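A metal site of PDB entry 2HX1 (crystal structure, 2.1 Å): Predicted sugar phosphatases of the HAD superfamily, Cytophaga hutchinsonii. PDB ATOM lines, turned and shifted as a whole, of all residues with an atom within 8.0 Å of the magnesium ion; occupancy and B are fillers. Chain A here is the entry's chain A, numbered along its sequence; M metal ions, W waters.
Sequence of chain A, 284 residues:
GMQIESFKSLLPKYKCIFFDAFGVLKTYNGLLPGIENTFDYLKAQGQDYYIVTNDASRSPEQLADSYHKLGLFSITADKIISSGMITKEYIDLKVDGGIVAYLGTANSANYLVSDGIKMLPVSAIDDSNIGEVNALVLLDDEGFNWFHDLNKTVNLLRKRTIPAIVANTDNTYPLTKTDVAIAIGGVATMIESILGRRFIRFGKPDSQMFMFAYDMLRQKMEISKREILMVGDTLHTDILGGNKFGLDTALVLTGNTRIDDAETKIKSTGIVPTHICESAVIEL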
ATOM      1  N   PHE A  19     -20.428   0.949   4.230  1.00  0.00           N
ATOM      2  CA  PHE A  19     -21.700   1.107   4.913  1.00  0.00           C
ATOM      3  C   PHE A  19     -22.710   0.066   4.400  1.00  0.00           C
ATOM      4  O   PHE A  19     -22.914  -0.014   3.213  1.00  0.00           O
ATOM      5  CB  PHE A  19     -22.290   2.491   4.624  1.00  0.00           C
ATOM      6  CG  PHE A  19     -21.614   3.646   5.343  1.00  0.00           C
ATOM      7  CD1 PHE A  19     -21.843   3.883   6.684  1.00  0.00           C
ATOM      8  CD2 PHE A  19     -20.801   4.504   4.660  1.00  0.00           C
ATOM      9  CE1 PHE A  19     -21.257   4.942   7.321  1.00  0.00           C
ATOM     10  CE2 PHE A  19     -20.205   5.567   5.307  1.00  0.00           C
ATOM     11  CZ  PHE A  19     -20.449   5.791   6.617  1.00  0.00           C
ATOM     12  N   ASP A  20     -23.288  -0.746   5.287  1.00  0.00           N
ATOM     13  CA  ASP A  20     -24.564  -1.379   5.027  1.00  0.00           C
ATOM     14  C   ASP A  20     -25.613  -0.256   4.923  1.00  0.00           C
ATOM     15  O   ASP A  20     -25.411   0.810   5.511  1.00  0.00           O
ATOM     16  CB  ASP A  20     -24.910  -2.361   6.154  1.00  0.00           C
ATOM     17  CG  ASP A  20     -26.300  -2.960   6.020  1.00  0.00           C
ATOM     18  OD1 ASP A  20     -26.684  -3.359   4.914  1.00  0.00           O
ATOM     19  OD2 ASP A  20     -27.016  -3.019   7.037  1.00  0.00           O
ATOM     20  N   ALA A  21     -26.707  -0.462   4.182  1.00  0.00           N
ATOM     21  CA  ALA A  21     -27.706   0.614   3.987  1.00  0.00           C
ATOM     22  C   ALA A  21     -28.830   0.474   5.019  1.00  0.00           C
ATOM     23  O   ALA A  21     -28.895   1.270   5.926  1.00  0.00           O
ATOM     24  CB  ALA A  21     -28.244   0.654   2.576  1.00  0.00           C
ATOM     25  N   PHE A  22     -29.643  -0.567   4.928  1.00  0.00           N
ATOM     26  CA  PHE A  22     -30.806  -0.683   5.806  1.00  0.00           C
ATOM     27  C   PHE A  22     -30.397  -0.990   7.261  1.00  0.00           C
ATOM     28  O   PHE A  22     -29.587  -1.896   7.521  1.00  0.00           O
ATOM     29  CB  PHE A  22     -31.828  -1.699   5.275  1.00  0.00           C
ATOM     30  CG  PHE A  22     -32.767  -1.134   4.231  1.00  0.00           C
ATOM     31  CD1 PHE A  22     -33.842  -0.347   4.597  1.00  0.00           C
ATOM     32  CD2 PHE A  22     -32.568  -1.398   2.869  1.00  0.00           C
ATOM     33  CE1 PHE A  22     -34.713   0.186   3.622  1.00  0.00           C
ATOM     34  CE2 PHE A  22     -33.432  -0.870   1.899  1.00  0.00           C
ATOM     35  CZ  PHE A  22     -34.507  -0.090   2.277  1.00  0.00           C
ATOM     36  N   GLY A  23     -30.950  -0.198   8.171  1.00  0.00           N
ATOM     37  CA  GLY A  23     -30.648  -0.260   9.593  1.00  0.00           C
ATOM     38  C   GLY A  23     -29.495   0.603  10.036  1.00  0.00           C
ATOM     39  O   GLY A  23     -29.189   0.673  11.232  1.00  0.00           O
ATOM     40  N   VAL A  24     -28.862   1.249   9.058  1.00  0.00           N
ATOM     41  CA  VAL A  24     -27.638   2.026   9.253  1.00  0.00           C
ATOM     42  C   VAL A  24     -27.792   3.440   8.655  1.00  0.00           C
ATOM     43  O   VAL A  24     -27.555   4.433   9.338  1.00  0.00           O
ATOM     44  CB  VAL A  24     -26.452   1.314   8.578  1.00  0.00           C
ATOM     45  CG1 VAL A  24     -25.143   2.089   8.753  1.00  0.00           C
ATOM     46  CG2 VAL A  24     -26.313  -0.144   9.136  1.00  0.00           C
ATOM     47  N   LEU A  25     -28.150   3.520   7.381  1.00  0.00           N
ATOM     48  CA  LEU A  25     -28.315   4.798   6.693  1.00  0.00           C
ATOM     49  C   LEU A  25     -29.782   5.184   6.572  1.00  0.00           C
ATOM     50  O   LEU A  25     -30.121   6.367   6.505  1.00  0.00           O
ATOM     51  CB  LEU A  25     -27.743   4.749   5.276  1.00  0.00           C
ATOM     52  CG  LEU A  25     -26.252   4.475   5.088  1.00  0.00           C
ATOM     53  CD1 LEU A  25     -25.934   4.484   3.588  1.00  0.00           C
ATOM     54  CD2 LEU A  25     -25.397   5.468   5.860  1.00  0.00           C
ATOM     55  N   LYS A  26     -30.646   4.173   6.539  1.00  0.00           N
ATOM     56  CA  LYS A  26     -32.072   4.390   6.341  1.00  0.00           C
ATOM     57  C   LYS A  26     -32.857   3.229   6.940  1.00  0.00           C
ATOM     58  O   LYS A  26     -32.290   2.183   7.243  1.00  0.00           O
ATOM     59  CB  LYS A  26     -32.381   4.573   4.848  1.00  0.00           C
ATOM     60  CG  LYS A  26     -32.038   3.373   3.980  1.00  0.00           C
ATOM     61  CD  LYS A  26     -32.378   3.667   2.516  1.00  0.00           C
ATOM     62  CE  LYS A  26     -32.123   2.487   1.613  1.00  0.00           C
ATOM     63  NZ  LYS A  26     -32.726   2.666   0.262  1.00  0.00           N
ATOM     64  N   VAL A  52     -22.229  -1.161   0.643  1.00  0.00           N
ATOM     65  CA  VAL A  52     -22.110  -2.575   0.318  1.00  0.00           C
ATOM     66  C   VAL A  52     -23.425  -3.188   0.850  1.00  0.00           C
ATOM     67  O   VAL A  52     -23.663  -3.222   2.068  1.00  0.00           O
ATOM     68  CB  VAL A  52     -20.894  -3.207   0.988  1.00  0.00           C
ATOM     69  CG1 VAL A  52     -20.825  -4.666   0.687  1.00  0.00           C
ATOM     70  CG2 VAL A  52     -19.634  -2.466   0.551  1.00  0.00           C
ATOM     71  N   THR A  53     -24.265  -3.623  -0.079  1.00  0.00           N
ATOM     72  CA  THR A  53     -25.623  -3.964   0.207  1.00  0.00           C
ATOM     73  C   THR A  53     -25.990  -5.279  -0.462  1.00  0.00           C
ATOM     74  O   THR A  53     -25.544  -5.558  -1.598  1.00  0.00           O
ATOM     75  CB  THR A  53     -26.547  -2.855  -0.286  1.00  0.00           C
ATOM     76  OG1 THR A  53     -27.920  -3.178   0.019  1.00  0.00           O
ATOM     77  CG2 THR A  53     -26.395  -2.626  -1.782  1.00  0.00           C
ATOM     78  N   ASP A 170     -31.836 -10.471   4.839  1.00  0.00           N
ATOM     79  CA  ASP A 170     -32.436 -10.921   6.068  1.00  0.00           C
ATOM     80  C   ASP A 170     -33.737 -11.608   5.659  1.00  0.00           C
ATOM     81  O   ASP A 170     -34.264 -11.328   4.602  1.00  0.00           O
ATOM     82  CB  ASP A 170     -32.718  -9.719   7.007  1.00  0.00           C
ATOM     83  CG  ASP A 170     -31.429  -8.940   7.402  1.00  0.00           C
ATOM     84  OD1 ASP A 170     -30.400  -9.593   7.753  1.00  0.00           O
ATOM     85  OD2 ASP A 170     -31.470  -7.666   7.401  1.00  0.00           O
ATOM     86  N   LYS A 204     -23.061 -10.510   1.486  1.00  0.00           N
ATOM     87  CA  LYS A 204     -22.559 -10.656   2.849  1.00  0.00           C
ATOM     88  C   LYS A 204     -23.296 -11.804   3.510  1.00  0.00           C
ATOM     89  O   LYS A 204     -24.506 -11.931   3.338  1.00  0.00           O
ATOM     90  CB  LYS A 204     -22.780  -9.350   3.650  1.00  0.00           C
ATOM     91  CG  LYS A 204     -22.240  -8.054   2.970  1.00  0.00           C
ATOM     92  CD  LYS A 204     -22.708  -6.806   3.706  1.00  0.00           C
ATOM     93  CE  LYS A 204     -24.177  -6.486   3.468  1.00  0.00           C
ATOM     94  NZ  LYS A 204     -24.534  -5.146   3.970  1.00  0.00           N
ATOM     95  N   MET A 230     -16.124  -1.697   8.199  1.00  0.00           N
ATOM     96  CA  MET A 230     -17.446  -2.160   7.775  1.00  0.00           C
ATOM     97  C   MET A 230     -18.434  -1.778   8.853  1.00  0.00           C
ATOM     98  O   MET A 230     -18.286  -2.185   9.996  1.00  0.00           O
ATOM     99  CB  MET A 230     -17.510  -3.684   7.555  1.00  0.00           C
ATOM    100  CG  MET A 230     -18.961  -4.231   7.379  1.00  0.00           C
ATOM    101  SD  MET A 230     -19.635  -3.798   5.612  1.00  0.00           S
ATOM    102  CE  MET A 230     -21.523  -3.406   5.812  1.00  0.00           C
ATOM    103  N   VAL A 231     -19.465  -1.015   8.473  1.00  0.00           N
ATOM    104  CA  VAL A 231     -20.472  -0.497   9.416  1.00  0.00           C
ATOM    105  C   VAL A 231     -21.808  -1.180   9.170  1.00  0.00           C
ATOM    106  O   VAL A 231     -22.375  -1.096   8.065  1.00  0.00           O
ATOM    107  CB  VAL A 231     -20.583   1.059   9.272  1.00  0.00           C
ATOM    108  CG1 VAL A 231     -21.634   1.621  10.199  1.00  0.00           C
ATOM    109  CG2 VAL A 231     -19.188   1.718   9.510  1.00  0.00           C
ATOM    110  N   GLY A 232     -22.320  -1.890  10.159  1.00  0.00           N
ATOM    111  CA  GLY A 232     -23.588  -2.599   9.971  1.00  0.00           C
ATOM    112  C   GLY A 232     -24.417  -2.804  11.233  1.00  0.00           C
ATOM    113  O   GLY A 232     -23.923  -2.614  12.344  1.00  0.00           O
ATOM    114  N   ASP A 233     -25.671  -3.194  11.031  1.00  0.00           N
ATOM    115  CA  ASP A 233     -26.598  -3.456  12.145  1.00  0.00           C
ATOM    116  C   ASP A 233     -26.860  -4.926  12.411  1.00  0.00           C
ATOM    117  O   ASP A 233     -27.529  -5.255  13.384  1.00  0.00           O
ATOM    118  CB  ASP A 233     -27.928  -2.728  11.924  1.00  0.00           C
ATOM    119  CG  ASP A 233     -28.664  -3.232  10.697  1.00  0.00           C
ATOM    120  OD1 ASP A 233     -28.022  -3.322   9.627  1.00  0.00           O
ATOM    121  OD2 ASP A 233     -29.877  -3.570  10.813  1.00  0.00           O
ATOM    122  N   THR A 234     -26.316  -5.808  11.565  1.00  0.00           N
ATOM    123  CA  THR A 234     -26.600  -7.243  11.624  1.00  0.00           C
ATOM    124  C   THR A 234     -25.334  -8.057  11.777  1.00  0.00           C
ATOM    125  O   THR A 234     -24.424  -7.935  10.958  1.00  0.00           O
ATOM    126  CB  THR A 234     -27.339  -7.661  10.348  1.00  0.00           C
ATOM    127  OG1 THR A 234     -28.493  -6.832  10.193  1.00  0.00           O
ATOM    128  CG2 THR A 234     -27.776  -9.165  10.399  1.00  0.00           C
ATOM    129  N   THR A 237     -24.364 -11.068   9.068  1.00  0.00           N
ATOM    130  CA  THR A 237     -24.066 -10.677   7.696  1.00  0.00           C
ATOM    131  C   THR A 237     -22.915  -9.618   7.618  1.00  0.00           C
ATOM    132  O   THR A 237     -21.786  -9.890   7.135  1.00  0.00           O
ATOM    133  CB  THR A 237     -25.341 -10.137   6.944  1.00  0.00           C
ATOM    134  OG1 THR A 237     -25.893  -9.025   7.649  1.00  0.00           O
ATOM    135  CG2 THR A 237     -26.454 -11.194   6.821  1.00  0.00           C
ATOM    136  N   ASP A 238     -23.196  -8.416   8.099  1.00  0.00           N
ATOM    137  CA  ASP A 238     -22.211  -7.328   8.099  1.00  0.00           C
ATOM    138  C   ASP A 238     -20.955  -7.577   8.951  1.00  0.00           C
ATOM    139  O   ASP A 238     -19.841  -7.405   8.476  1.00  0.00           O
ATOM    140  CB  ASP A 238     -22.856  -6.021   8.574  1.00  0.00           C
ATOM    141  CG  ASP A 238     -24.147  -5.717   7.856  1.00  0.00           C
ATOM    142  OD1 ASP A 238     -24.197  -5.889   6.607  1.00  0.00           O
ATOM    143  OD2 ASP A 238     -25.122  -5.359   8.535  1.00  0.00           O
ATOM    144  N   VAL A 252     -23.600  -0.858  14.596  1.00  0.00           N
ATOM    145  CA  VAL A 252     -24.529   0.214  15.008  1.00  0.00           C
ATOM    146  C   VAL A 252     -25.805  -0.360  15.600  1.00  0.00           C
ATOM    147  O   VAL A 252     -26.185  -1.509  15.327  1.00  0.00           O
ATOM    148  CB  VAL A 252     -24.857   1.197  13.908  1.00  0.00           C
ATOM    149  CG1 VAL A 252     -23.636   2.030  13.627  1.00  0.00           C
ATOM    150  CG2 VAL A 252     -25.396   0.497  12.660  1.00  0.00           C
ATOM    151  N   THR A 254     -28.926   0.967  15.446  1.00  0.00           N
ATOM    152  CA  THR A 254     -30.075   1.588  14.848  1.00  0.00           C
ATOM    153  C   THR A 254     -30.929   0.630  14.030  1.00  0.00           C
ATOM    154  O   THR A 254     -31.876   1.071  13.378  1.00  0.00           O
ATOM    155  CB  THR A 254     -29.672   2.789  13.959  1.00  0.00           C
ATOM    156  OG1 THR A 254     -28.559   2.433  13.117  1.00  0.00           O
ATOM    157  CG2 THR A 254     -29.299   3.996  14.827  1.00  0.00           C
ATOM    158  N   GLY A 255     -30.630  -0.657  14.074  1.00  0.00           N
ATOM    159  CA  GLY A 255     -31.290  -1.627  13.197  1.00  0.00           C
ATOM    160  C   GLY A 255     -31.620  -2.934  13.874  1.00  0.00           C
ATOM    161  O   GLY A 255     -32.190  -2.932  14.960  1.00  0.00           O
ATOM    162  N   ASN A 256     -31.248  -4.051  13.251  1.00  0.00           N
ATOM    163  CA  ASN A 256     -31.565  -5.385  13.753  1.00  0.00           C
ATOM    164  C   ASN A 256     -31.009  -5.706  15.132  1.00  0.00           C
ATOM    165  O   ASN A 256     -31.538  -6.581  15.783  1.00  0.00           O
ATOM    166  CB  ASN A 256     -31.058  -6.487  12.813  1.00  0.00           C
ATOM    167  CG  ASN A 256     -31.885  -6.615  11.520  1.00  0.00           C
ATOM    168  OD1 ASN A 256     -33.071  -6.285  11.464  1.00  0.00           O
ATOM    169  ND2 ASN A 256     -31.221  -7.092  10.463  1.00  0.00           N
HETATM  170 MG    MG M   1     -28.729  -3.710   7.707  1.00  0.00          MG
HETATM  171  O   HOH W   1     -27.659  -5.570   7.757  1.00  0.00           O
HETATM  172  O   HOH W   2     -29.180  -4.057   5.729  1.00  0.00           O
HETATM  173  O   HOH W   3     -30.520  -4.395   8.277  1.00  0.00           O
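Water W1 lies within hydrogen-bond range of the side-chain carboxylate (OD2) of Asp 238 and the side-chain hydroxyl (OG1) of Thr 234.
N of Asn 256 lies within hydrogen-bond range of OD2 of Asp 233, 2.8 Å away. The side-chain carboxylate (OD1) of Asp 20 lies within salt-bridge range of the side-chain amino group (NZ) of Lys 204. OD2 of Asp 238 is in hydrogen-bond range of N of Asp 233 (3.3 Å). The backbone NH (N) of Thr 234 is in hydrogen-bond range of the side-chain carboxylate (OD2) of Asp 238, 3.3 Å away. The backbone NH (N) of Asp 20 is in hydrogen-bond range of the backbone carbonyl oxygen (O) of Val 231 (2.9 Å). OG1 of Thr 234 sits at hydrogen-bond distance from ND2 of Asn 256 (2.8 Å).
The magnesium ion is bound by the side-chain carboxylate (OD2) of Asp 20 (2.0 Å), water W3 (2.0 Å), the backbone carbonyl oxygen (O) of Phe 22 (2.0 Å), water W2 (2.1 Å), the side-chain carboxylate (OD1) of Asp 233 (2.1 Å) and water W1 (2.1 Å).
OG1 of Thr 234 touches the magnesium ion (3.998 Å).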
